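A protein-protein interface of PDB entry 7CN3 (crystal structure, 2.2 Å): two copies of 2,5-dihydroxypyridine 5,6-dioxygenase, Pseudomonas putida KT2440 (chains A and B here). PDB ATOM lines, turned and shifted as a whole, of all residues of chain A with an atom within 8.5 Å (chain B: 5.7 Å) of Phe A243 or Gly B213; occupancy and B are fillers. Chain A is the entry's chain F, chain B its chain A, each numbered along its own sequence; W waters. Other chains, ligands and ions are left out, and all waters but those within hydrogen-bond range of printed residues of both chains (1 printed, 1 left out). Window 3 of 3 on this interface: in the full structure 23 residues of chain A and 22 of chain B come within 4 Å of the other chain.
The guanidinium group (NH2) of Arg B224 lies within salt-bridge range of the side-chain carboxylate (OE1) of Glu A225 (3.0 Å).
The guanidinium group (NH1) of Arg B224 is in salt-bridge range of the side-chain carboxylate (OE2) of Glu A244, at 3.0 Å.
The side-chain carboxylate of Asp A250 is in salt-bridge range of the guanidinium group of Arg B324.
The backbone carbonyl oxygen (O) of Gly B213 lies within hydrogen-bond range of the indole nitrogen (NE1) of Trp B276, at 2.9 Å.
The backbone NH (N) of Gly B213 is in hydrogen-bond range of the backbone carbonyl oxygen (O) of Cys B223 (2.7 Å).
The backbone carbonyl oxygen of Trp B276 lies within hydrogen-bond range of the side-chain hydroxyl of Tyr B222, at 2.7 Å.
OE1 of Glu A225 sits at hydrogen-bond distance from N of Phe A243, 2.9 Å away.
The backbone NH (N) of Glu A225 is in hydrogen-bond range of the side-chain carboxylate (OE1) of Glu A244 (3.4 Å).
The side-chain carboxylate (OD1) of Asp B214 is in hydrogen-bond range of the backbone NH (N) of Arg B324.
Among the printed residues, pairs that only touch across the chains: Tyr A247 with Tyr B222, Phe A243 with Tyr B222, Phe A243 with Gly B213, Phe A243 with Trp B276, Phe A243 with Arg B224, Phe A243 with Val B212 and Asp A250 with Trp B276.
Of chain B, only Val B212 (3.8 Å), Gly B213 (3.6 Å), Tyr B222 (3.5 Å), Arg B224 (3.7 Å) and Trp B276 (3.6 Å) come within 4 Å of Phe A243.
Of chain A, only Phe A243 comes within 4 Å of Gly B213.
Of the printed residues of chain A, Trp B276 touches Phe A243 (3.6 Å) and Asp A250 (3.9 Å).
Of the printed residues of chain B, Glu A244 touches Arg B224.
Of the printed residues of chain A, Arg B224 touches Glu A225 (3.0 Å), Phe A243 (3.7 Å) and Glu A244 (3.0 Å).
The nearest residue of chain B that does not touch Phe A243 is Cys B223 (5.1 Å).
The nearest residue of chain A that does not touch Gly B213 is Glu A246 (5.7 Å).
Hydrophobic or aromatic side chains of chain B within 4 Å of the printed part of chain A: Val B212, Tyr B222 and Trp B276.
Of the 19 printed residues of chain A, 5 touch a printed residue of chain B.
Printed residues of chain A that touch a printed residue of chain B: Glu A225, Phe A243, Glu A244, Tyr A247 and Asp A250.
Hydrophobic or aromatic side chains of chain A that line the printed part of chain B: Phe A243 and Tyr A247.
Among the printed residues, Asp or Glu carboxylates within 4 Å of a Lys or Arg side-chain nitrogen of the other chain: Glu A225 with Arg B224 (3.0 Å), Glu A244 with Arg B224 (3.0 Å) and Asp A250 with Arg B324 (3.3 Å).
Positions printed for both chains: 223 and 224.
Water W1 bridges the side-chain carboxylate of Asp A250 and the backbone NH of Trp B276.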
ATOM      1  N   PHE A 219       9.988  18.461  11.242  1.00  0.00           N
ATOM      2  CA  PHE A 219      11.360  18.777  10.828  1.00  0.00           C
ATOM      3  C   PHE A 219      11.550  20.280  10.683  1.00  0.00           C
ATOM      4  O   PHE A 219      12.630  20.806  10.956  1.00  0.00           O
ATOM      5  CB  PHE A 219      11.733  18.101   9.501  1.00  0.00           C
ATOM      6  CG  PHE A 219      11.569  16.607   9.486  1.00  0.00           C
ATOM      7  CD1 PHE A 219      11.365  15.885  10.651  1.00  0.00           C
ATOM      8  CD2 PHE A 219      11.636  15.922   8.274  1.00  0.00           C
ATOM      9  CE1 PHE A 219      11.207  14.504  10.609  1.00  0.00           C
ATOM     10  CE2 PHE A 219      11.487  14.536   8.218  1.00  0.00           C
ATOM     11  CZ  PHE A 219      11.274  13.831   9.380  1.00  0.00           C
ATOM     12  N   ASN A 221      11.696  22.157   7.900  1.00  0.00           N
ATOM     13  CA  ASN A 221      12.594  22.540   6.815  1.00  0.00           C
ATOM     14  C   ASN A 221      11.776  22.792   5.561  1.00  0.00           C
ATOM     15  O   ASN A 221      10.750  22.145   5.343  1.00  0.00           O
ATOM     16  CB  ASN A 221      13.640  21.449   6.522  1.00  0.00           C
ATOM     17  CG  ASN A 221      14.413  21.041   7.755  1.00  0.00           C
ATOM     18  OD1 ASN A 221      14.913  21.887   8.494  1.00  0.00           O
ATOM     19  ND2 ASN A 221      14.497  19.741   7.998  1.00  0.00           N
ATOM     20  N   CYS A 223      11.837  21.944   1.849  1.00  0.00           N
ATOM     21  CA  CYS A 223      12.541  20.977   1.004  1.00  0.00           C
ATOM     22  C   CYS A 223      13.329  21.698  -0.081  1.00  0.00           C
ATOM     23  O   CYS A 223      12.795  22.557  -0.784  1.00  0.00           O
ATOM     24  CB  CYS A 223      11.576  19.990   0.361  1.00  0.00           C
ATOM     25  SG  CYS A 223      10.658  18.951   1.549  1.00  0.00           S
ATOM     26  N   ARG A 224      14.611  21.368  -0.208  1.00  0.00           N
ATOM     27  CA  ARG A 224      15.410  21.876  -1.311  1.00  0.00           C
ATOM     28  C   ARG A 224      15.501  20.886  -2.466  1.00  0.00           C
ATOM     29  O   ARG A 224      15.923  21.277  -3.556  1.00  0.00           O
ATOM     30  CB  ARG A 224      16.814  22.248  -0.819  1.00  0.00           C
ATOM     31  CG  ARG A 224      16.795  23.238   0.356  1.00  0.00           C
ATOM     32  CD  ARG A 224      16.114  24.562  -0.040  1.00  0.00           C
ATOM     33  NE  ARG A 224      16.694  25.174  -1.245  1.00  0.00           N
ATOM     34  CZ  ARG A 224      17.541  26.212  -1.241  1.00  0.00           C
ATOM     35  NH1 ARG A 224      17.925  26.763  -0.103  1.00  0.00           N
ATOM     36  NH2 ARG A 224      18.010  26.701  -2.382  1.00  0.00           N
ATOM     37  N   GLU A 225      15.119  19.624  -2.246  1.00  0.00           N
ATOM     38  CA  GLU A 225      14.929  18.633  -3.305  1.00  0.00           C
ATOM     39  C   GLU A 225      13.570  17.970  -3.123  1.00  0.00           C
ATOM     40  O   GLU A 225      13.066  17.867  -2.001  1.00  0.00           O
ATOM     41  CB  GLU A 225      16.013  17.555  -3.288  1.00  0.00           C
ATOM     42  CG  GLU A 225      17.437  18.065  -3.410  1.00  0.00           C
ATOM     43  CD  GLU A 225      18.447  16.945  -3.221  1.00  0.00           C
ATOM     44  OE1 GLU A 225      18.520  16.388  -2.102  1.00  0.00           O
ATOM     45  OE2 GLU A 225      19.146  16.600  -4.202  1.00  0.00           O
ATOM     46  N   ARG A 226      12.990  17.502  -4.228  1.00  0.00           N
ATOM     47  CA  ARG A 226      11.657  16.916  -4.177  1.00  0.00           C
ATOM     48  C   ARG A 226      11.655  15.583  -3.436  1.00  0.00           C
ATOM     49  O   ARG A 226      12.643  14.842  -3.429  1.00  0.00           O
ATOM     50  CB  ARG A 226      11.093  16.701  -5.584  1.00  0.00           C
ATOM     51  CG  ARG A 226      10.936  17.957  -6.393  1.00  0.00           C
ATOM     52  CD  ARG A 226      10.244  17.629  -7.701  1.00  0.00           C
ATOM     53  NE  ARG A 226       9.729  18.828  -8.359  1.00  0.00           N
ATOM     54  CZ  ARG A 226       9.164  18.831  -9.565  1.00  0.00           C
ATOM     55  NH1 ARG A 226       9.042  17.692 -10.246  1.00  0.00           N
ATOM     56  NH2 ARG A 226       8.722  19.971 -10.089  1.00  0.00           N
ATOM     57  N   ILE A 227      10.512  15.280  -2.821  1.00  0.00           N
ATOM     58  CA  ILE A 227      10.220  13.970  -2.254  1.00  0.00           C
ATOM     59  C   ILE A 227       8.939  13.459  -2.896  1.00  0.00           C
ATOM     60  O   ILE A 227       7.916  14.157  -2.898  1.00  0.00           O
ATOM     61  CB  ILE A 227      10.045  14.017  -0.727  1.00  0.00           C
ATOM     62  CG1 ILE A 227      11.252  14.645  -0.041  1.00  0.00           C
ATOM     63  CG2 ILE A 227       9.768  12.597  -0.180  1.00  0.00           C
ATOM     64  CD1 ILE A 227      11.171  14.552   1.493  1.00  0.00           C
ATOM     65  N   ILE A 239       9.083   6.098  -0.742  1.00  0.00           N
ATOM     66  CA  ILE A 239       9.583   7.441  -0.435  1.00  0.00           C
ATOM     67  C   ILE A 239      10.863   7.629  -1.238  1.00  0.00           C
ATOM     68  O   ILE A 239      11.870   6.965  -0.968  1.00  0.00           O
ATOM     69  CB  ILE A 239       9.844   7.644   1.070  1.00  0.00           C
ATOM     70  CG1 ILE A 239       8.583   7.360   1.891  1.00  0.00           C
ATOM     71  CG2 ILE A 239      10.330   9.074   1.357  1.00  0.00           C
ATOM     72  CD1 ILE A 239       8.790   7.537   3.398  1.00  0.00           C
ATOM     73  N   HIS A 240      10.832   8.532  -2.216  1.00  0.00           N
ATOM     74  CA  HIS A 240      11.917   8.642  -3.180  1.00  0.00           C
ATOM     75  C   HIS A 240      12.336  10.091  -3.365  1.00  0.00           C
ATOM     76  O   HIS A 240      11.506  11.004  -3.339  1.00  0.00           O
ATOM     77  CB  HIS A 240      11.512   8.060  -4.536  1.00  0.00           C
ATOM     78  CG  HIS A 240      11.021   6.647  -4.459  1.00  0.00           C
ATOM     79  ND1 HIS A 240       9.681   6.317  -4.489  1.00  0.00           N
ATOM     80  CD2 HIS A 240      11.694   5.478  -4.336  1.00  0.00           C
ATOM     81  CE1 HIS A 240       9.549   5.006  -4.397  1.00  0.00           C
ATOM     82  NE2 HIS A 240      10.755   4.473  -4.303  1.00  0.00           N
ATOM     83  N   GLY A 241      13.623  10.286  -3.575  1.00  0.00           N
ATOM     84  CA  GLY A 241      14.137  11.589  -3.933  1.00  0.00           C
ATOM     85  C   GLY A 241      15.563  11.760  -3.429  1.00  0.00           C
ATOM     86  O   GLY A 241      16.383  10.847  -3.545  1.00  0.00           O
ATOM     87  N   GLY A 242      15.831  12.927  -2.863  1.00  0.00           N
ATOM     88  CA  GLY A 242      17.185  13.316  -2.506  1.00  0.00           C
ATOM     89  C   GLY A 242      17.502  13.111  -1.038  1.00  0.00           C
ATOM     90  O   GLY A 242      17.097  12.120  -0.419  1.00  0.00           O
ATOM     91  N   PHE A 243      18.274  14.047  -0.483  1.00  0.00           N
ATOM     92  CA  PHE A 243      18.675  13.927   0.913  1.00  0.00           C
ATOM     93  C   PHE A 243      17.469  13.952   1.847  1.00  0.00           C
ATOM     94  O   PHE A 243      17.410  13.183   2.812  1.00  0.00           O
ATOM     95  CB  PHE A 243      19.653  15.041   1.284  1.00  0.00           C
ATOM     96  CG  PHE A 243      19.794  15.219   2.748  1.00  0.00           C
ATOM     97  CD1 PHE A 243      20.458  14.267   3.504  1.00  0.00           C
ATOM     98  CD2 PHE A 243      19.197  16.281   3.388  1.00  0.00           C
ATOM     99  CE1 PHE A 243      20.557  14.400   4.868  1.00  0.00           C
ATOM    100  CE2 PHE A 243      19.297  16.425   4.753  1.00  0.00           C
ATOM    101  CZ  PHE A 243      19.973  15.483   5.494  1.00  0.00           C
ATOM    102  N   GLU A 244      16.515  14.852   1.599  1.00  0.00           N
ATOM    103  CA  GLU A 244      15.334  14.919   2.452  1.00  0.00           C
ATOM    104  C   GLU A 244      14.596  13.587   2.469  1.00  0.00           C
ATOM    105  O   GLU A 244      14.060  13.171   3.510  1.00  0.00           O
ATOM    106  CB  GLU A 244      14.400  16.034   1.979  1.00  0.00           C
ATOM    107  CG  GLU A 244      14.777  17.439   2.415  1.00  0.00           C
ATOM    108  CD  GLU A 244      15.526  18.196   1.336  1.00  0.00           C
ATOM    109  OE1 GLU A 244      15.913  17.578   0.324  1.00  0.00           O
ATOM    110  OE2 GLU A 244      15.748  19.409   1.504  1.00  0.00           O
ATOM    111  N   ALA A 245      14.551  12.901   1.321  1.00  0.00           N
ATOM    112  CA  ALA A 245      13.885  11.604   1.279  1.00  0.00           C
ATOM    113  C   ALA A 245      14.583  10.613   2.193  1.00  0.00           C
ATOM    114  O   ALA A 245      13.926   9.885   2.945  1.00  0.00           O
ATOM    115  CB  ALA A 245      13.836  11.072  -0.159  1.00  0.00           C
ATOM    116  N   GLU A 246      15.924  10.589   2.150  1.00  0.00           N
ATOM    117  CA  GLU A 246      16.699   9.672   2.984  1.00  0.00           C
ATOM    118  C   GLU A 246      16.533   9.992   4.461  1.00  0.00           C
ATOM    119  O   GLU A 246      16.368   9.088   5.289  1.00  0.00           O
ATOM    120  CB  GLU A 246      18.182   9.729   2.610  1.00  0.00           C
ATOM    121  CG  GLU A 246      19.055   8.919   3.561  1.00  0.00           C
ATOM    122  CD  GLU A 246      20.487   8.800   3.099  1.00  0.00           C
ATOM    123  OE1 GLU A 246      21.034   9.803   2.610  1.00  0.00           O
ATOM    124  OE2 GLU A 246      21.063   7.700   3.222  1.00  0.00           O
ATOM    125  N   TYR A 247      16.608  11.278   4.809  1.00  0.00           N
ATOM    126  CA  TYR A 247      16.378  11.689   6.183  1.00  0.00           C
ATOM    127  C   TYR A 247      15.002  11.235   6.642  1.00  0.00           C
ATOM    128  O   TYR A 247      14.857  10.619   7.704  1.00  0.00           O
ATOM    129  CB  TYR A 247      16.528  13.215   6.299  1.00  0.00           C
ATOM    130  CG  TYR A 247      16.364  13.746   7.701  1.00  0.00           C
ATOM    131  CD1 TYR A 247      15.103  13.973   8.234  1.00  0.00           C
ATOM    132  CD2 TYR A 247      17.469  14.012   8.497  1.00  0.00           C
ATOM    133  CE1 TYR A 247      14.952  14.453   9.516  1.00  0.00           C
ATOM    134  CE2 TYR A 247      17.324  14.503   9.795  1.00  0.00           C
ATOM    135  CZ  TYR A 247      16.066  14.719  10.290  1.00  0.00           C
ATOM    136  OH  TYR A 247      15.911  15.188  11.571  1.00  0.00           O
ATOM    137  N   LEU A 248      13.983  11.511   5.825  1.00  0.00           N
ATOM    138  CA  LEU A 248      12.621  11.126   6.170  1.00  0.00           C
ATOM    139  C   LEU A 248      12.484   9.609   6.293  1.00  0.00           C
ATOM    140  O   LEU A 248      11.841   9.116   7.230  1.00  0.00           O
ATOM    141  CB  LEU A 248      11.646  11.690   5.127  1.00  0.00           C
ATOM    142  CG  LEU A 248      10.203  11.173   5.221  1.00  0.00           C
ATOM    143  CD1 LEU A 248       9.524  11.743   6.454  1.00  0.00           C
ATOM    144  CD2 LEU A 248       9.400  11.490   3.961  1.00  0.00           C
ATOM    145  N   ARG A 249      13.068   8.852   5.348  1.00  0.00           N
ATOM    146  CA  ARG A 249      13.023   7.390   5.422  1.00  0.00           C
ATOM    147  C   ARG A 249      13.659   6.900   6.715  1.00  0.00           C
ATOM    148  O   ARG A 249      13.094   6.064   7.423  1.00  0.00           O
ATOM    149  CB  ARG A 249      13.736   6.762   4.214  1.00  0.00           C
ATOM    150  CG  ARG A 249      12.837   6.441   3.028  1.00  0.00           C
ATOM    151  CD  ARG A 249      13.572   5.601   1.974  1.00  0.00           C
ATOM    152  NE  ARG A 249      14.968   6.005   1.776  1.00  0.00           N
ATOM    153  CZ  ARG A 249      15.385   6.819   0.808  1.00  0.00           C
ATOM    154  NH1 ARG A 249      14.515   7.329  -0.060  1.00  0.00           N
ATOM    155  NH2 ARG A 249      16.671   7.136   0.704  1.00  0.00           N
ATOM    156  N   ASP A 250      14.841   7.422   7.028  1.00  0.00           N
ATOM    157  CA  ASP A 250      15.527   7.071   8.262  1.00  0.00           C
ATOM    158  C   ASP A 250      14.682   7.430   9.483  1.00  0.00           C
ATOM    159  O   ASP A 250      14.565   6.633  10.421  1.00  0.00           O
ATOM    160  CB  ASP A 250      16.880   7.786   8.280  1.00  0.00           C
ATOM    161  CG  ASP A 250      17.868   7.183   9.251  1.00  0.00           C
ATOM    162  OD1 ASP A 250      17.782   7.513  10.448  1.00  0.00           O
ATOM    163  OD2 ASP A 250      18.753   6.414   8.812  1.00  0.00           O
ATOM    164  N   ASP B 211      30.187  13.157   2.671  1.00  0.00           N
ATOM    165  CA  ASP B 211      29.111  12.956   1.713  1.00  0.00           C
ATOM    166  C   ASP B 211      27.907  13.827   2.071  1.00  0.00           C
ATOM    167  O   ASP B 211      27.819  14.398   3.161  1.00  0.00           O
ATOM    168  CB  ASP B 211      28.706  11.486   1.687  1.00  0.00           C
ATOM    169  CG  ASP B 211      27.932  11.103   0.433  1.00  0.00           C
ATOM    170  OD1 ASP B 211      27.871  11.913  -0.520  1.00  0.00           O
ATOM    171  OD2 ASP B 211      27.386   9.976   0.415  1.00  0.00           O
ATOM    172  N   VAL B 212      26.983  13.939   1.114  1.00  0.00           N
ATOM    173  CA  VAL B 212      25.650  14.457   1.391  1.00  0.00           C
ATOM    174  C   VAL B 212      25.095  13.770   2.633  1.00  0.00           C
ATOM    175  O   VAL B 212      25.098  12.538   2.732  1.00  0.00           O
ATOM    176  CB  VAL B 212      24.748  14.239   0.160  1.00  0.00           C
ATOM    177  CG1 VAL B 212      23.283  14.442   0.501  1.00  0.00           C
ATOM    178  CG2 VAL B 212      25.175  15.178  -0.980  1.00  0.00           C
ATOM    179  N   GLY B 213      24.640  14.566   3.600  1.00  0.00           N
ATOM    180  CA  GLY B 213      24.110  14.035   4.839  1.00  0.00           C
ATOM    181  C   GLY B 213      25.104  13.949   5.986  1.00  0.00           C
ATOM    182  O   GLY B 213      24.682  13.788   7.138  1.00  0.00           O
ATOM    183  N   ASP B 214      26.402  14.042   5.710  1.00  0.00           N
ATOM    184  CA  ASP B 214      27.372  14.003   6.794  1.00  0.00           C
ATOM    185  C   ASP B 214      27.433  15.364   7.500  1.00  0.00           C
ATOM    186  O   ASP B 214      26.883  16.364   7.028  1.00  0.00           O
ATOM    187  CB  ASP B 214      28.735  13.559   6.271  1.00  0.00           C
ATOM    188  CG  ASP B 214      28.778  12.056   5.971  1.00  0.00           C
ATOM    189  OD1 ASP B 214      27.951  11.308   6.533  1.00  0.00           O
ATOM    190  OD2 ASP B 214      29.636  11.622   5.176  1.00  0.00           O
ATOM    191  N   ILE B 215      28.094  15.388   8.662  1.00  0.00           N
ATOM    192  CA  ILE B 215      27.913  16.445   9.652  1.00  0.00           C
ATOM    193  C   ILE B 215      29.257  17.024  10.067  1.00  0.00           C
ATOM    194  O   ILE B 215      30.211  16.278  10.308  1.00  0.00           O
ATOM    195  CB  ILE B 215      27.168  15.916  10.902  1.00  0.00           C
ATOM    196  CG1 ILE B 215      25.818  15.302  10.511  1.00  0.00           C
ATOM    197  CG2 ILE B 215      27.040  17.020  11.957  1.00  0.00           C
ATOM    198  CD1 ILE B 215      25.020  14.729  11.706  1.00  0.00           C
ATOM    199  N   TYR B 222      23.691  19.246   8.111  1.00  0.00           N
ATOM    200  CA  TYR B 222      23.853  18.117   7.197  1.00  0.00           C
ATOM    201  C   TYR B 222      24.395  18.658   5.869  1.00  0.00           C
ATOM    202  O   TYR B 222      23.772  19.539   5.262  1.00  0.00           O
ATOM    203  CB  TYR B 222      22.520  17.395   6.972  1.00  0.00           C
ATOM    204  CG  TYR B 222      21.870  16.809   8.224  1.00  0.00           C
ATOM    205  CD1 TYR B 222      22.225  15.546   8.685  1.00  0.00           C
ATOM    206  CD2 TYR B 222      20.923  17.520   8.942  1.00  0.00           C
ATOM    207  CE1 TYR B 222      21.646  15.002   9.822  1.00  0.00           C
ATOM    208  CE2 TYR B 222      20.323  16.983  10.089  1.00  0.00           C
ATOM    209  CZ  TYR B 222      20.693  15.720  10.522  1.00  0.00           C
ATOM    210  OH  TYR B 222      20.134  15.165  11.651  1.00  0.00           O
ATOM    211  N   CYS B 223      25.551  18.158   5.428  1.00  0.00           N
ATOM    212  CA  CYS B 223      26.106  18.592   4.146  1.00  0.00           C
ATOM    213  C   CYS B 223      25.144  18.293   3.008  1.00  0.00           C
ATOM    214  O   CYS B 223      24.595  17.188   2.910  1.00  0.00           O
ATOM    215  CB  CYS B 223      27.446  17.907   3.858  1.00  0.00           C
ATOM    216  SG  CYS B 223      28.798  18.371   4.919  1.00  0.00           S
ATOM    217  N   ARG B 224      24.942  19.292   2.148  1.00  0.00           N
ATOM    218  CA  ARG B 224      24.130  19.135   0.954  1.00  0.00           C
ATOM    219  C   ARG B 224      24.971  18.946  -0.305  1.00  0.00           C
ATOM    220  O   ARG B 224      24.421  18.594  -1.357  1.00  0.00           O
ATOM    221  CB  ARG B 224      23.190  20.342   0.807  1.00  0.00           C
ATOM    222  CG  ARG B 224      22.266  20.524   2.013  1.00  0.00           C
ATOM    223  CD  ARG B 224      21.443  19.246   2.290  1.00  0.00           C
ATOM    224  NE  ARG B 224      20.647  18.823   1.130  1.00  0.00           N
ATOM    225  CZ  ARG B 224      19.341  19.060   0.982  1.00  0.00           C
ATOM    226  NH1 ARG B 224      18.672  19.722   1.919  1.00  0.00           N
ATOM    227  NH2 ARG B 224      18.698  18.652  -0.112  1.00  0.00           N
ATOM    228  N   TRP B 276      21.372   9.721  14.069  1.00  0.00           N
ATOM    229  CA  TRP B 276      21.864  10.641  13.052  1.00  0.00           C
ATOM    230  C   TRP B 276      20.832  11.709  12.698  1.00  0.00           C
ATOM    231  O   TRP B 276      21.202  12.846  12.387  1.00  0.00           O
ATOM    232  CB  TRP B 276      22.267   9.832  11.811  1.00  0.00           C
ATOM    233  CG  TRP B 276      22.489  10.648  10.576  1.00  0.00           C
ATOM    234  CD1 TRP B 276      23.570  11.443  10.292  1.00  0.00           C
ATOM    235  CD2 TRP B 276      21.617  10.744   9.449  1.00  0.00           C
ATOM    236  NE1 TRP B 276      23.417  12.026   9.054  1.00  0.00           N
ATOM    237  CE2 TRP B 276      22.225  11.616   8.518  1.00  0.00           C
ATOM    238  CE3 TRP B 276      20.383  10.167   9.128  1.00  0.00           C
ATOM    239  CZ2 TRP B 276      21.641  11.929   7.298  1.00  0.00           C
ATOM    240  CZ3 TRP B 276      19.807  10.475   7.915  1.00  0.00           C
ATOM    241  CH2 TRP B 276      20.437  11.350   7.014  1.00  0.00           C
ATOM    242  N   ARG B 324      28.717   8.753   7.657  1.00  0.00           N
ATOM    243  CA  ARG B 324      27.837   7.599   7.488  1.00  0.00           C
ATOM    244  C   ARG B 324      28.403   6.617   6.457  1.00  0.00           C
ATOM    245  O   ARG B 324      29.282   6.952   5.663  1.00  0.00           O
ATOM    246  CB  ARG B 324      26.443   8.038   7.037  1.00  0.00           C
ATOM    247  CG  ARG B 324      25.663   8.887   8.049  1.00  0.00           C
ATOM    248  CD  ARG B 324      24.144   8.866   7.772  1.00  0.00           C
ATOM    249  NE  ARG B 324      23.663   7.533   7.397  1.00  0.00           N
ATOM    250  CZ  ARG B 324      22.621   6.904   7.953  1.00  0.00           C
ATOM    251  NH1 ARG B 324      21.926   7.477   8.928  1.00  0.00           N
ATOM    252  NH2 ARG B 324      22.280   5.682   7.544  1.00  0.00           N
HETATM  253  O   HOH W   1      18.931   8.328  12.639  1.00  0.00           O
